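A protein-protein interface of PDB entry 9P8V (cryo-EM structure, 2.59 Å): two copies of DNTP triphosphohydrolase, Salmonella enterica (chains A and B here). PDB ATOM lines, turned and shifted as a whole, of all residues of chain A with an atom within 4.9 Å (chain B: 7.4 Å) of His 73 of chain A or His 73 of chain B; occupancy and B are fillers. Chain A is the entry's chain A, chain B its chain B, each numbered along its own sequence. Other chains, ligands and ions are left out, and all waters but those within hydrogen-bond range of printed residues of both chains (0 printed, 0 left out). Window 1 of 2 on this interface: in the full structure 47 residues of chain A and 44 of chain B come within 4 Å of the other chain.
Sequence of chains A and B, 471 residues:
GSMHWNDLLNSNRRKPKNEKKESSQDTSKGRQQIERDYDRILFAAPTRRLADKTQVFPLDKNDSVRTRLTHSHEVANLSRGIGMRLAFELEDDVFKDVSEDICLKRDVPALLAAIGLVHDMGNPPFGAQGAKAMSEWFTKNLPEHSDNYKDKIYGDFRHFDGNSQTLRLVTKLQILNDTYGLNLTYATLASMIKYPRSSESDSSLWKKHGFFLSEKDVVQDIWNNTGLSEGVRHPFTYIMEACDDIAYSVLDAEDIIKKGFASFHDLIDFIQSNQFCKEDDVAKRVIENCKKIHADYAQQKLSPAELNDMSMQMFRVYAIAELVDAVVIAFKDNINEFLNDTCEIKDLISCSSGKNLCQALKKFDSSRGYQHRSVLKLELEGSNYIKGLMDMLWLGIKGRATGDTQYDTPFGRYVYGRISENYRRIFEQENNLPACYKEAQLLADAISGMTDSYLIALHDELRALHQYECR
A ring nitrogen (NE2) of His 73 of chain B lies close to a ring nitrogen (ND1) of His 73 of chain A, at 3.4 Å.
NH2 of Arg 48 of chain B is in hydrogen-bond range of O of Phe 43 of chain B.
Among the printed residues, merely in contact across the chains: Tyr 38 of chain A with Asn 77 of chain B (3.3 Å), Asn 77 of chain A with Tyr 38 of chain B (3.3 Å), Leu 42 of chain A with Asn 77 of chain B (3.6 Å), Glu 74 of chain A with Leu 42 of chain B (3.6 Å), Thr 70 of chain A with Arg 48 of chain B (3.7 Å), Glu 74 of chain A with Phe 43 of chain B (3.7 Å), Asn 77 of chain A with Leu 42 of chain B (3.7 Å), Leu 42 of chain A with His 73 of chain B (3.9 Å) and Asn 77 of chain A with Phe 43 of chain B (3.9 Å).
Printed residues of chain B within 4 Å of His 73 of chain A: His 73 (3.2 Å). His 73 of chain B touches just these residues of chain A: Leu 42 and His 73. Of the printed residues of chain B, Tyr 38 of chain A touches Asn 77 (3.3 Å). Of the printed residues of chain A, Arg 48 of chain B touches Thr 70. Printed residues of chain B within 4 Å of Leu 42 of chain A: His 73 (3.9 Å) and Asn 77 (3.6 Å). Printed residues of chain A within 4 Å of Asn 77 of chain B: Tyr 38 (3.3 Å) and Leu 42 (3.6 Å). Val 75 of chain B touches none of the printed residues of chain A. Arg 68 of chain B touches none of the printed residues of chain A. The nearest residue of chain B that does not touch His 73 of chain A is Leu 42 of chain B (4.2 Å). The nearest printed residue of chain A that does not touch Phe 43 of chain B is Val 75 of chain A (6.5 Å).
Hydrophobic or aromatic side chains of chain A that line the printed part of chain B: Tyr 38, Leu 42 and His 73. Hydrophobic or aromatic side chains of chain B that line the printed part of chain A: Tyr 38, Leu 42, Phe 43 and His 73.
Tyr 38 of chain A touches Asn 77 of chain B, and with the chains exchanged Asn 77 of chain A touches Tyr 38 of chain B. Leu 42 of chain A touches His 73 of chain B, but with the chains exchanged His 73 of chain A does not touch Leu 42 of chain B (4.2 Å). Leu 42 of chain A touches Asn 77 of chain B, and with the chains exchanged Asn 77 of chain A touches Leu 42 of chain B. His 73 of chain B touches its own counterpart, His 73 of chain A.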
ATOM      1  N   TYR A  38      38.931  -7.899  19.396  1.00  0.00           N
ATOM      2  CA  TYR A  38      37.659  -8.516  19.757  1.00  0.00           C
ATOM      3  C   TYR A  38      37.720  -9.127  21.150  1.00  0.00           C
ATOM      4  O   TYR A  38      36.761  -9.024  21.924  1.00  0.00           O
ATOM      5  CB  TYR A  38      37.274  -9.574  18.723  1.00  0.00           C
ATOM      6  CG  TYR A  38      35.905 -10.178  18.943  1.00  0.00           C
ATOM      7  CD1 TYR A  38      34.766  -9.555  18.457  1.00  0.00           C
ATOM      8  CD2 TYR A  38      35.751 -11.371  19.632  1.00  0.00           C
ATOM      9  CE1 TYR A  38      33.515 -10.099  18.652  1.00  0.00           C
ATOM     10  CE2 TYR A  38      34.501 -11.923  19.834  1.00  0.00           C
ATOM     11  CZ  TYR A  38      33.387 -11.283  19.341  1.00  0.00           C
ATOM     12  OH  TYR A  38      32.139 -11.826  19.535  1.00  0.00           O
ATOM     13  N   LEU A  42      35.378  -7.985  24.240  1.00  0.00           N
ATOM     14  CA  LEU A  42      34.472  -8.957  24.844  1.00  0.00           C
ATOM     15  C   LEU A  42      34.743  -9.129  26.333  1.00  0.00           C
ATOM     16  O   LEU A  42      33.804  -9.222  27.133  1.00  0.00           O
ATOM     17  CB  LEU A  42      34.589 -10.297  24.121  1.00  0.00           C
ATOM     18  CG  LEU A  42      33.692 -11.417  24.645  1.00  0.00           C
ATOM     19  CD1 LEU A  42      32.228 -11.028  24.540  1.00  0.00           C
ATOM     20  CD2 LEU A  42      33.961 -12.706  23.893  1.00  0.00           C
ATOM     21  N   THR A  47      31.022  -4.540  28.387  1.00  0.00           N
ATOM     22  CA  THR A  47      30.341  -5.527  27.555  1.00  0.00           C
ATOM     23  C   THR A  47      29.419  -6.404  28.392  1.00  0.00           C
ATOM     24  O   THR A  47      28.277  -6.666  28.000  1.00  0.00           O
ATOM     25  CB  THR A  47      31.365  -6.382  26.809  1.00  0.00           C
ATOM     26  OG1 THR A  47      32.184  -5.540  25.989  1.00  0.00           O
ATOM     27  CG2 THR A  47      30.665  -7.404  25.928  1.00  0.00           C
ATOM     28  N   LEU A  69      23.130  -6.219  25.335  1.00  0.00           N
ATOM     29  CA  LEU A  69      24.193  -7.181  25.056  1.00  0.00           C
ATOM     30  C   LEU A  69      23.794  -8.146  23.948  1.00  0.00           C
ATOM     31  O   LEU A  69      24.595  -8.449  23.057  1.00  0.00           O
ATOM     32  CB  LEU A  69      24.555  -7.950  26.325  1.00  0.00           C
ATOM     33  CG  LEU A  69      25.657  -8.997  26.168  1.00  0.00           C
ATOM     34  CD1 LEU A  69      26.934  -8.342  25.681  1.00  0.00           C
ATOM     35  CD2 LEU A  69      25.893  -9.734  27.473  1.00  0.00           C
ATOM     36  N   THR A  70      22.564  -8.663  24.002  1.00  0.00           N
ATOM     37  CA  THR A  70      22.102  -9.560  22.949  1.00  0.00           C
ATOM     38  C   THR A  70      22.039  -8.847  21.607  1.00  0.00           C
ATOM     39  O   THR A  70      22.429  -9.416  20.581  1.00  0.00           O
ATOM     40  CB  THR A  70      20.733 -10.134  23.309  1.00  0.00           C
ATOM     41  OG1 THR A  70      19.822  -9.064  23.582  1.00  0.00           O
ATOM     42  CG2 THR A  70      20.840 -11.019  24.536  1.00  0.00           C
ATOM     43  N   HIS A  71      21.562  -7.601  21.598  1.00  0.00           N
ATOM     44  CA  HIS A  71      21.557  -6.818  20.369  1.00  0.00           C
ATOM     45  C   HIS A  71      22.970  -6.610  19.846  1.00  0.00           C
ATOM     46  O   HIS A  71      23.214  -6.718  18.639  1.00  0.00           O
ATOM     47  CB  HIS A  71      20.878  -5.472  20.610  1.00  0.00           C
ATOM     48  CG  HIS A  71      21.204  -4.440  19.577  1.00  0.00           C
ATOM     49  ND1 HIS A  71      20.554  -4.372  18.365  1.00  0.00           N
ATOM     50  CD2 HIS A  71      22.123  -3.445  19.567  1.00  0.00           C
ATOM     51  CE1 HIS A  71      21.048  -3.372  17.658  1.00  0.00           C
ATOM     52  NE2 HIS A  71      22.003  -2.795  18.364  1.00  0.00           N
ATOM     53  N   SER A  72      23.913  -6.302  20.738  1.00  0.00           N
ATOM     54  CA  SER A  72      25.292  -6.087  20.316  1.00  0.00           C
ATOM     55  C   SER A  72      25.889  -7.354  19.719  1.00  0.00           C
ATOM     56  O   SER A  72      26.565  -7.305  18.686  1.00  0.00           O
ATOM     57  CB  SER A  72      26.131  -5.600  21.496  1.00  0.00           C
ATOM     58  OG  SER A  72      25.677  -4.338  21.954  1.00  0.00           O
ATOM     59  N   HIS A  73      25.645  -8.502  20.352  1.00  0.00           N
ATOM     60  CA  HIS A  73      26.173  -9.756  19.822  1.00  0.00           C
ATOM     61  C   HIS A  73      25.536 -10.119  18.490  1.00  0.00           C
ATOM     62  O   HIS A  73      26.217 -10.641  17.602  1.00  0.00           O
ATOM     63  CB  HIS A  73      25.976 -10.887  20.828  1.00  0.00           C
ATOM     64  CG  HIS A  73      27.071 -10.985  21.842  1.00  0.00           C
ATOM     65  ND1 HIS A  73      28.266 -11.619  21.585  1.00  0.00           N
ATOM     66  CD2 HIS A  73      27.152 -10.529  23.114  1.00  0.00           C
ATOM     67  CE1 HIS A  73      29.039 -11.548  22.654  1.00  0.00           C
ATOM     68  NE2 HIS A  73      28.385 -10.892  23.597  1.00  0.00           N
ATOM     69  N   GLU A  74      24.239  -9.861  18.330  1.00  0.00           N
ATOM     70  CA  GLU A  74      23.583 -10.142  17.060  1.00  0.00           C
ATOM     71  C   GLU A  74      24.086  -9.222  15.949  1.00  0.00           C
ATOM     72  O   GLU A  74      24.293  -9.675  14.814  1.00  0.00           O
ATOM     73  CB  GLU A  74      22.072 -10.037  17.259  1.00  0.00           C
ATOM     74  CG  GLU A  74      21.447 -11.373  17.631  1.00  0.00           C
ATOM     75  CD  GLU A  74      20.384 -11.260  18.708  1.00  0.00           C
ATOM     76  OE1 GLU A  74      19.491 -10.403  18.591  1.00  0.00           O
ATOM     77  OE2 GLU A  74      20.443 -12.041  19.679  1.00  0.00           O
ATOM     78  N   VAL A  75      24.319  -7.945  16.264  1.00  0.00           N
ATOM     79  CA  VAL A  75      24.935  -7.034  15.304  1.00  0.00           C
ATOM     80  C   VAL A  75      26.333  -7.512  14.939  1.00  0.00           C
ATOM     81  O   VAL A  75      26.734  -7.469  13.770  1.00  0.00           O
ATOM     82  CB  VAL A  75      24.959  -5.601  15.865  1.00  0.00           C
ATOM     83  CG1 VAL A  75      25.841  -4.707  15.010  1.00  0.00           C
ATOM     84  CG2 VAL A  75      23.558  -5.037  15.941  1.00  0.00           C
ATOM     85  N   ALA A  76      27.101  -7.963  15.933  1.00  0.00           N
ATOM     86  CA  ALA A  76      28.444  -8.465  15.669  1.00  0.00           C
ATOM     87  C   ALA A  76      28.407  -9.694  14.773  1.00  0.00           C
ATOM     88  O   ALA A  76      29.247  -9.844  13.882  1.00  0.00           O
ATOM     89  CB  ALA A  76      29.154  -8.782  16.983  1.00  0.00           C
ATOM     90  N   ASN A  77      27.445 -10.590  15.002  1.00  0.00           N
ATOM     91  CA  ASN A  77      27.322 -11.772  14.156  1.00  0.00           C
ATOM     92  C   ASN A  77      26.966 -11.395  12.724  1.00  0.00           C
ATOM     93  O   ASN A  77      27.522 -11.954  11.770  1.00  0.00           O
ATOM     94  CB  ASN A  77      26.277 -12.724  14.733  1.00  0.00           C
ATOM     95  CG  ASN A  77      25.922 -13.843  13.780  1.00  0.00           C
ATOM     96  OD1 ASN A  77      24.776 -13.969  13.354  1.00  0.00           O
ATOM     97  ND2 ASN A  77      26.908 -14.665  13.439  1.00  0.00           N
ATOM     98  N   LEU A 117      30.306  -5.459  17.898  1.00  0.00           N
ATOM     99  CA  LEU A 117      30.183  -5.725  19.328  1.00  0.00           C
ATOM    100  C   LEU A 117      30.413  -4.464  20.150  1.00  0.00           C
ATOM    101  O   LEU A 117      29.722  -4.234  21.148  1.00  0.00           O
ATOM    102  CB  LEU A 117      31.166  -6.817  19.745  1.00  0.00           C
ATOM    103  CG  LEU A 117      31.081  -7.279  21.199  1.00  0.00           C
ATOM    104  CD1 LEU A 117      29.680  -7.755  21.530  1.00  0.00           C
ATOM    105  CD2 LEU A 117      32.101  -8.365  21.478  1.00  0.00           C
ATOM    106  N   TYR B  38      25.631 -21.409  13.612  1.00  0.00           N
ATOM    107  CA  TYR B  38      25.921 -20.411  14.634  1.00  0.00           C
ATOM    108  C   TYR B  38      24.815 -19.369  14.716  1.00  0.00           C
ATOM    109  O   TYR B  38      24.424 -18.954  15.813  1.00  0.00           O
ATOM    110  CB  TYR B  38      27.266 -19.744  14.357  1.00  0.00           C
ATOM    111  CG  TYR B  38      27.681 -18.752  15.421  1.00  0.00           C
ATOM    112  CD1 TYR B  38      28.338 -19.170  16.569  1.00  0.00           C
ATOM    113  CD2 TYR B  38      27.417 -17.398  15.276  1.00  0.00           C
ATOM    114  CE1 TYR B  38      28.717 -18.269  17.542  1.00  0.00           C
ATOM    115  CE2 TYR B  38      27.793 -16.490  16.245  1.00  0.00           C
ATOM    116  CZ  TYR B  38      28.442 -16.930  17.375  1.00  0.00           C
ATOM    117  OH  TYR B  38      28.819 -16.029  18.343  1.00  0.00           O
ATOM    118  N   LEU B  42      22.530 -18.649  17.954  1.00  0.00           N
ATOM    119  CA  LEU B  42      22.566 -17.326  18.569  1.00  0.00           C
ATOM    120  C   LEU B  42      21.182 -16.695  18.623  1.00  0.00           C
ATOM    121  O   LEU B  42      20.826 -16.050  19.616  1.00  0.00           O
ATOM    122  CB  LEU B  42      23.539 -16.426  17.810  1.00  0.00           C
ATOM    123  CG  LEU B  42      23.690 -14.998  18.329  1.00  0.00           C
ATOM    124  CD1 LEU B  42      24.869 -14.895  19.279  1.00  0.00           C
ATOM    125  CD2 LEU B  42      23.852 -14.033  17.171  1.00  0.00           C
ATOM    126  N   PHE B  43      20.385 -16.866  17.571  1.00  0.00           N
ATOM    127  CA  PHE B  43      19.055 -16.271  17.545  1.00  0.00           C
ATOM    128  C   PHE B  43      18.020 -17.092  18.303  1.00  0.00           C
ATOM    129  O   PHE B  43      16.870 -16.654  18.414  1.00  0.00           O
ATOM    130  CB  PHE B  43      18.598 -16.059  16.101  1.00  0.00           C
ATOM    131  CG  PHE B  43      19.206 -14.852  15.447  1.00  0.00           C
ATOM    132  CD1 PHE B  43      18.619 -13.607  15.587  1.00  0.00           C
ATOM    133  CD2 PHE B  43      20.361 -14.960  14.693  1.00  0.00           C
ATOM    134  CE1 PHE B  43      19.173 -12.493  14.989  1.00  0.00           C
ATOM    135  CE2 PHE B  43      20.919 -13.849  14.093  1.00  0.00           C
ATOM    136  CZ  PHE B  43      20.325 -12.614  14.241  1.00  0.00           C
ATOM    137  N   THR B  47      19.361 -19.114  24.116  1.00  0.00           N
ATOM    138  CA  THR B  47      20.684 -18.499  24.103  1.00  0.00           C
ATOM    139  C   THR B  47      20.669 -17.165  24.837  1.00  0.00           C
ATOM    140  O   THR B  47      21.558 -16.878  25.646  1.00  0.00           O
ATOM    141  CB  THR B  47      21.164 -18.321  22.662  1.00  0.00           C
ATOM    142  OG1 THR B  47      21.603 -19.583  22.146  1.00  0.00           O
ATOM    143  CG2 THR B  47      22.313 -17.329  22.594  1.00  0.00           C
ATOM    144  N   ARG B  48      19.655 -16.341  24.582  1.00  0.00           N
ATOM    145  CA  ARG B  48      19.537 -15.074  25.288  1.00  0.00           C
ATOM    146  C   ARG B  48      18.844 -15.207  26.637  1.00  0.00           C
ATOM    147  O   ARG B  48      18.941 -14.285  27.454  1.00  0.00           O
ATOM    148  CB  ARG B  48      18.802 -14.054  24.415  1.00  0.00           C
ATOM    149  CG  ARG B  48      17.297 -14.086  24.532  1.00  0.00           C
ATOM    150  CD  ARG B  48      16.672 -13.205  23.470  1.00  0.00           C
ATOM    151  NE  ARG B  48      17.017 -13.651  22.126  1.00  0.00           N
ATOM    152  CZ  ARG B  48      16.148 -14.157  21.261  1.00  0.00           C
ATOM    153  NH1 ARG B  48      14.870 -14.297  21.568  1.00  0.00           N
ATOM    154  NH2 ARG B  48      16.574 -14.531  20.059  1.00  0.00           N
ATOM    155  N   LEU B  50      19.957 -17.423  28.608  1.00  0.00           N
ATOM    156  CA  LEU B  50      21.135 -17.728  29.411  1.00  0.00           C
ATOM    157  C   LEU B  50      21.658 -16.509  30.160  1.00  0.00           C
ATOM    158  O   LEU B  50      22.413 -16.669  31.124  1.00  0.00           O
ATOM    159  CB  LEU B  50      22.244 -18.297  28.525  1.00  0.00           C
ATOM    160  CG  LEU B  50      22.067 -19.726  28.016  1.00  0.00           C
ATOM    161  CD1 LEU B  50      23.316 -20.189  27.285  1.00  0.00           C
ATOM    162  CD2 LEU B  50      21.733 -20.666  29.159  1.00  0.00           C
ATOM    163  N   THR B  67      27.640 -14.341  33.926  1.00  0.00           N
ATOM    164  CA  THR B  67      26.448 -15.164  33.898  1.00  0.00           C
ATOM    165  C   THR B  67      26.672 -16.301  32.907  1.00  0.00           C
ATOM    166  O   THR B  67      27.770 -16.481  32.374  1.00  0.00           O
ATOM    167  CB  THR B  67      25.223 -14.322  33.539  1.00  0.00           C
ATOM    168  OG1 THR B  67      25.341 -13.860  32.189  1.00  0.00           O
ATOM    169  CG2 THR B  67      25.106 -13.130  34.470  1.00  0.00           C
ATOM    170  N   ARG B  68      25.628 -17.086  32.653  1.00  0.00           N
ATOM    171  CA  ARG B  68      25.777 -18.202  31.730  1.00  0.00           C
ATOM    172  C   ARG B  68      25.949 -17.734  30.289  1.00  0.00           C
ATOM    173  O   ARG B  68      26.679 -18.370  29.522  1.00  0.00           O
ATOM    174  CB  ARG B  68      24.581 -19.147  31.852  1.00  0.00           C
ATOM    175  CG  ARG B  68      24.790 -20.484  31.173  1.00  0.00           C
ATOM    176  CD  ARG B  68      25.814 -21.318  31.923  1.00  0.00           C
ATOM    177  NE  ARG B  68      25.399 -21.608  33.290  1.00  0.00           N
ATOM    178  CZ  ARG B  68      26.073 -22.383  34.126  1.00  0.00           C
ATOM    179  NH1 ARG B  68      27.200 -22.975  33.764  1.00  0.00           N
ATOM    180  NH2 ARG B  68      25.610 -22.567  35.359  1.00  0.00           N
ATOM    181  N   LEU B  69      25.305 -16.628  29.908  1.00  0.00           N
ATOM    182  CA  LEU B  69      25.440 -16.132  28.540  1.00  0.00           C
ATOM    183  C   LEU B  69      26.835 -15.577  28.286  1.00  0.00           C
ATOM    184  O   LEU B  69      27.437 -15.842  27.240  1.00  0.00           O
ATOM    185  CB  LEU B  69      24.383 -15.067  28.256  1.00  0.00           C
ATOM    186  CG  LEU B  69      24.476 -14.394  26.885  1.00  0.00           C
ATOM    187  CD1 LEU B  69      24.463 -15.430  25.774  1.00  0.00           C
ATOM    188  CD2 LEU B  69      23.354 -13.391  26.695  1.00  0.00           C
ATOM    189  N   THR B  70      27.362 -14.788  29.225  1.00  0.00           N
ATOM    190  CA  THR B  70      28.718 -14.274  29.069  1.00  0.00           C
ATOM    191  C   THR B  70      29.739 -15.402  29.083  1.00  0.00           C
ATOM    192  O   THR B  70      30.711 -15.371  28.318  1.00  0.00           O
ATOM    193  CB  THR B  70      29.029 -13.259  30.167  1.00  0.00           C
ATOM    194  OG1 THR B  70      28.975 -13.904  31.444  1.00  0.00           O
ATOM    195  CG2 THR B  70      28.020 -12.124  30.138  1.00  0.00           C
ATOM    196  N   HIS B  71      29.531 -16.403  29.938  1.00  0.00           N
ATOM    197  CA  HIS B  71      30.394 -17.579  29.942  1.00  0.00           C
ATOM    198  C   HIS B  71      30.364 -18.282  28.591  1.00  0.00           C
ATOM    199  O   HIS B  71      31.409 -18.654  28.046  1.00  0.00           O
ATOM    200  CB  HIS B  71      29.955 -18.531  31.053  1.00  0.00           C
ATOM    201  CG  HIS B  71      30.613 -19.874  30.997  1.00  0.00           C
ATOM    202  ND1 HIS B  71      31.975 -20.029  30.869  1.00  0.00           N
ATOM    203  CD2 HIS B  71      30.094 -21.123  31.043  1.00  0.00           C
ATOM    204  CE1 HIS B  71      32.268 -21.316  30.849  1.00  0.00           C
ATOM    205  NE2 HIS B  71      31.144 -22.002  30.951  1.00  0.00           N
ATOM    206  N   SER B  72      29.163 -18.468  28.036  1.00  0.00           N
ATOM    207  CA  SER B  72      29.037 -19.133  26.745  1.00  0.00           C
ATOM    208  C   SER B  72      29.716 -18.332  25.645  1.00  0.00           C
ATOM    209  O   SER B  72      30.378 -18.903  24.772  1.00  0.00           O
ATOM    210  CB  SER B  72      27.563 -19.353  26.414  1.00  0.00           C
ATOM    211  OG  SER B  72      26.934 -20.149  27.403  1.00  0.00           O
ATOM    212  N   HIS B  73      29.563 -17.008  25.664  1.00  0.00           N
ATOM    213  CA  HIS B  73      30.187 -16.180  24.639  1.00  0.00           C
ATOM    214  C   HIS B  73      31.706 -16.213  24.747  1.00  0.00           C
ATOM    215  O   HIS B  73      32.408 -16.253  23.730  1.00  0.00           O
ATOM    216  CB  HIS B  73      29.668 -14.747  24.732  1.00  0.00           C
ATOM    217  CG  HIS B  73      28.393 -14.521  23.983  1.00  0.00           C
ATOM    218  ND1 HIS B  73      28.150 -15.076  22.746  1.00  0.00           N
ATOM    219  CD2 HIS B  73      27.289 -13.806  24.297  1.00  0.00           C
ATOM    220  CE1 HIS B  73      26.952 -14.709  22.329  1.00  0.00           C
ATOM    221  NE2 HIS B  73      26.408 -13.937  23.252  1.00  0.00           N
ATOM    222  N   GLU B  74      32.235 -16.197  25.972  1.00  0.00           N
ATOM    223  CA  GLU B  74      33.681 -16.297  26.147  1.00  0.00           C
ATOM    224  C   GLU B  74      34.203 -17.648  25.671  1.00  0.00           C
ATOM    225  O   GLU B  74      35.256 -17.724  25.024  1.00  0.00           O
ATOM    226  CB  GLU B  74      34.046 -16.060  27.610  1.00  0.00           C
ATOM    227  CG  GLU B  74      34.282 -14.601  27.951  1.00  0.00           C
ATOM    228  CD  GLU B  74      33.758 -14.230  29.323  1.00  0.00           C
ATOM    229  OE1 GLU B  74      33.920 -15.037  30.262  1.00  0.00           O
ATOM    230  OE2 GLU B  74      33.186 -13.129  29.466  1.00  0.00           O
ATOM    231  N   VAL B  75      33.476 -18.726  25.981  1.00  0.00           N
ATOM    232  CA  VAL B  75      33.870 -20.051  25.508  1.00  0.00           C
ATOM    233  C   VAL B  75      33.839 -20.101  23.988  1.00  0.00           C
ATOM    234  O   VAL B  75      34.731 -20.675  23.352  1.00  0.00           O
ATOM    235  CB  VAL B  75      32.966 -21.130  26.130  1.00  0.00           C
ATOM    236  CG1 VAL B  75      33.175 -22.465  25.438  1.00  0.00           C
ATOM    237  CG2 VAL B  75      33.246 -21.258  27.608  1.00  0.00           C
ATOM    238  N   ALA B  76      32.812 -19.504  23.382  1.00  0.00           N
ATOM    239  CA  ALA B  76      32.716 -19.476  21.928  1.00  0.00           C
ATOM    240  C   ALA B  76      33.873 -18.701  21.316  1.00  0.00           C
ATOM    241  O   ALA B  76      34.424 -19.108  20.290  1.00  0.00           O
ATOM    242  CB  ALA B  76      31.381 -18.871  21.501  1.00  0.00           C
ATOM    243  N   ASN B  77      34.250 -17.576  21.925  1.00  0.00           N
ATOM    244  CA  ASN B  77      35.375 -16.803  21.408  1.00  0.00           C
ATOM    245  C   ASN B  77      36.679 -17.585  21.507  1.00  0.00           C
ATOM    246  O   ASN B  77      37.485 -17.584  20.568  1.00  0.00           O
ATOM    247  CB  ASN B  77      35.490 -15.477  22.155  1.00  0.00           C
ATOM    248  CG  ASN B  77      36.731 -14.703  21.772  1.00  0.00           C
ATOM    249  OD1 ASN B  77      36.895 -14.300  20.622  1.00  0.00           O
ATOM    250  ND2 ASN B  77      37.618 -14.492  22.737  1.00  0.00           N
ATOM    251  N   LEU B  78      36.905 -18.258  22.638  1.00  0.00           N
ATOM    252  CA  LEU B  78      38.118 -19.060  22.781  1.00  0.00           C
ATOM    253  C   LEU B  78      38.145 -20.202  21.773  1.00  0.00           C
ATOM    254  O   LEU B  78      39.187 -20.486  21.165  1.00  0.00           O
ATOM    255  CB  LEU B  78      38.225 -19.598  24.206  1.00  0.00           C
ATOM    256  CG  LEU B  78      38.495 -18.560  25.295  1.00  0.00           C
ATOM    257  CD1 LEU B  78      38.613 -19.231  26.648  1.00  0.00           C
ATOM    258  CD2 LEU B  78      39.752 -17.771  24.980  1.00  0.00           C
ATOM    259  N   SER B  79      37.005 -20.869  21.579  1.00  0.00           N
ATOM    260  CA  SER B  79      36.934 -21.955  20.611  1.00  0.00           C
ATOM    261  C   SER B  79      37.157 -21.443  19.196  1.00  0.00           C
ATOM    262  O   SER B  79      37.808 -22.110  18.385  1.00  0.00           O
ATOM    263  CB  SER B  79      35.589 -22.667  20.720  1.00  0.00           C
ATOM    264  OG  SER B  79      35.349 -23.093  22.049  1.00  0.00           O
ATOM    265  N   ALA B 113      33.038 -22.154  17.299  1.00  0.00           N
ATOM    266  CA  ALA B 113      32.322 -21.058  17.943  1.00  0.00           C
ATOM    267  C   ALA B 113      30.891 -21.452  18.280  1.00  0.00           C
ATOM    268  O   ALA B 113      30.408 -21.175  19.384  1.00  0.00           O
ATOM    269  CB  ALA B 113      32.342 -19.824  17.045  1.00  0.00           C
ATOM    270  N   GLY B 116      30.925 -23.948  21.195  1.00  0.00           N
ATOM    271  CA  GLY B 116      31.165 -23.279  22.462  1.00  0.00           C
ATOM    272  C   GLY B 116      29.976 -22.461  22.930  1.00  0.00           C
ATOM    273  O   GLY B 116      29.664 -22.432  24.123  1.00  0.00           O
ATOM    274  N   LEU B 117      29.298 -21.784  21.999  1.00  0.00           N
ATOM    275  CA  LEU B 117      28.136 -20.983  22.368  1.00  0.00           C
ATOM    276  C   LEU B 117      26.975 -21.854  22.826  1.00  0.00           C
ATOM    277  O   LEU B 117      26.185 -21.434  23.679  1.00  0.00           O
ATOM    278  CB  LEU B 117      27.711 -20.112  21.187  1.00  0.00           C
ATOM    279  CG  LEU B 117      26.480 -19.225  21.375  1.00  0.00           C
ATOM    280  CD1 LEU B 117      26.691 -18.254  22.523  1.00  0.00           C
ATOM    281  CD2 LEU B 117      26.155 -18.481  20.093  1.00  0.00           C
ATOM    282  N   HIS B 119      27.221 -24.844  24.318  1.00  0.00           N
ATOM    283  CA  HIS B 119      27.630 -25.877  25.263  1.00  0.00           C
ATOM    284  C   HIS B 119      26.844 -25.851  26.569  1.00  0.00           C
ATOM    285  O   HIS B 119      26.795 -26.872  27.262  1.00  0.00           O
ATOM    286  CB  HIS B 119      29.127 -25.750  25.549  1.00  0.00           C
ATOM    287  CG  HIS B 119      29.451 -24.899  26.736  1.00  0.00           C
ATOM    288  ND1 HIS B 119      29.560 -23.527  26.663  1.00  0.00           N
ATOM    289  CD2 HIS B 119      29.709 -25.228  28.024  1.00  0.00           C
ATOM    290  CE1 HIS B 119      29.861 -23.047  27.855  1.00  0.00           C
ATOM    291  NE2 HIS B 119      29.957 -24.057  28.700  1.00  0.00           N
ATOM    292  N   ALA B 247      37.819 -21.140  30.461  1.00  0.00           N
ATOM    293  CA  ALA B 247      37.014 -19.934  30.533  1.00  0.00           C
ATOM    294  C   ALA B 247      36.142 -19.870  31.772  1.00  0.00           C
ATOM    295  O   ALA B 247      35.630 -18.792  32.084  1.00  0.00           O
ATOM    296  CB  ALA B 247      36.138 -19.813  29.285  1.00  0.00           C
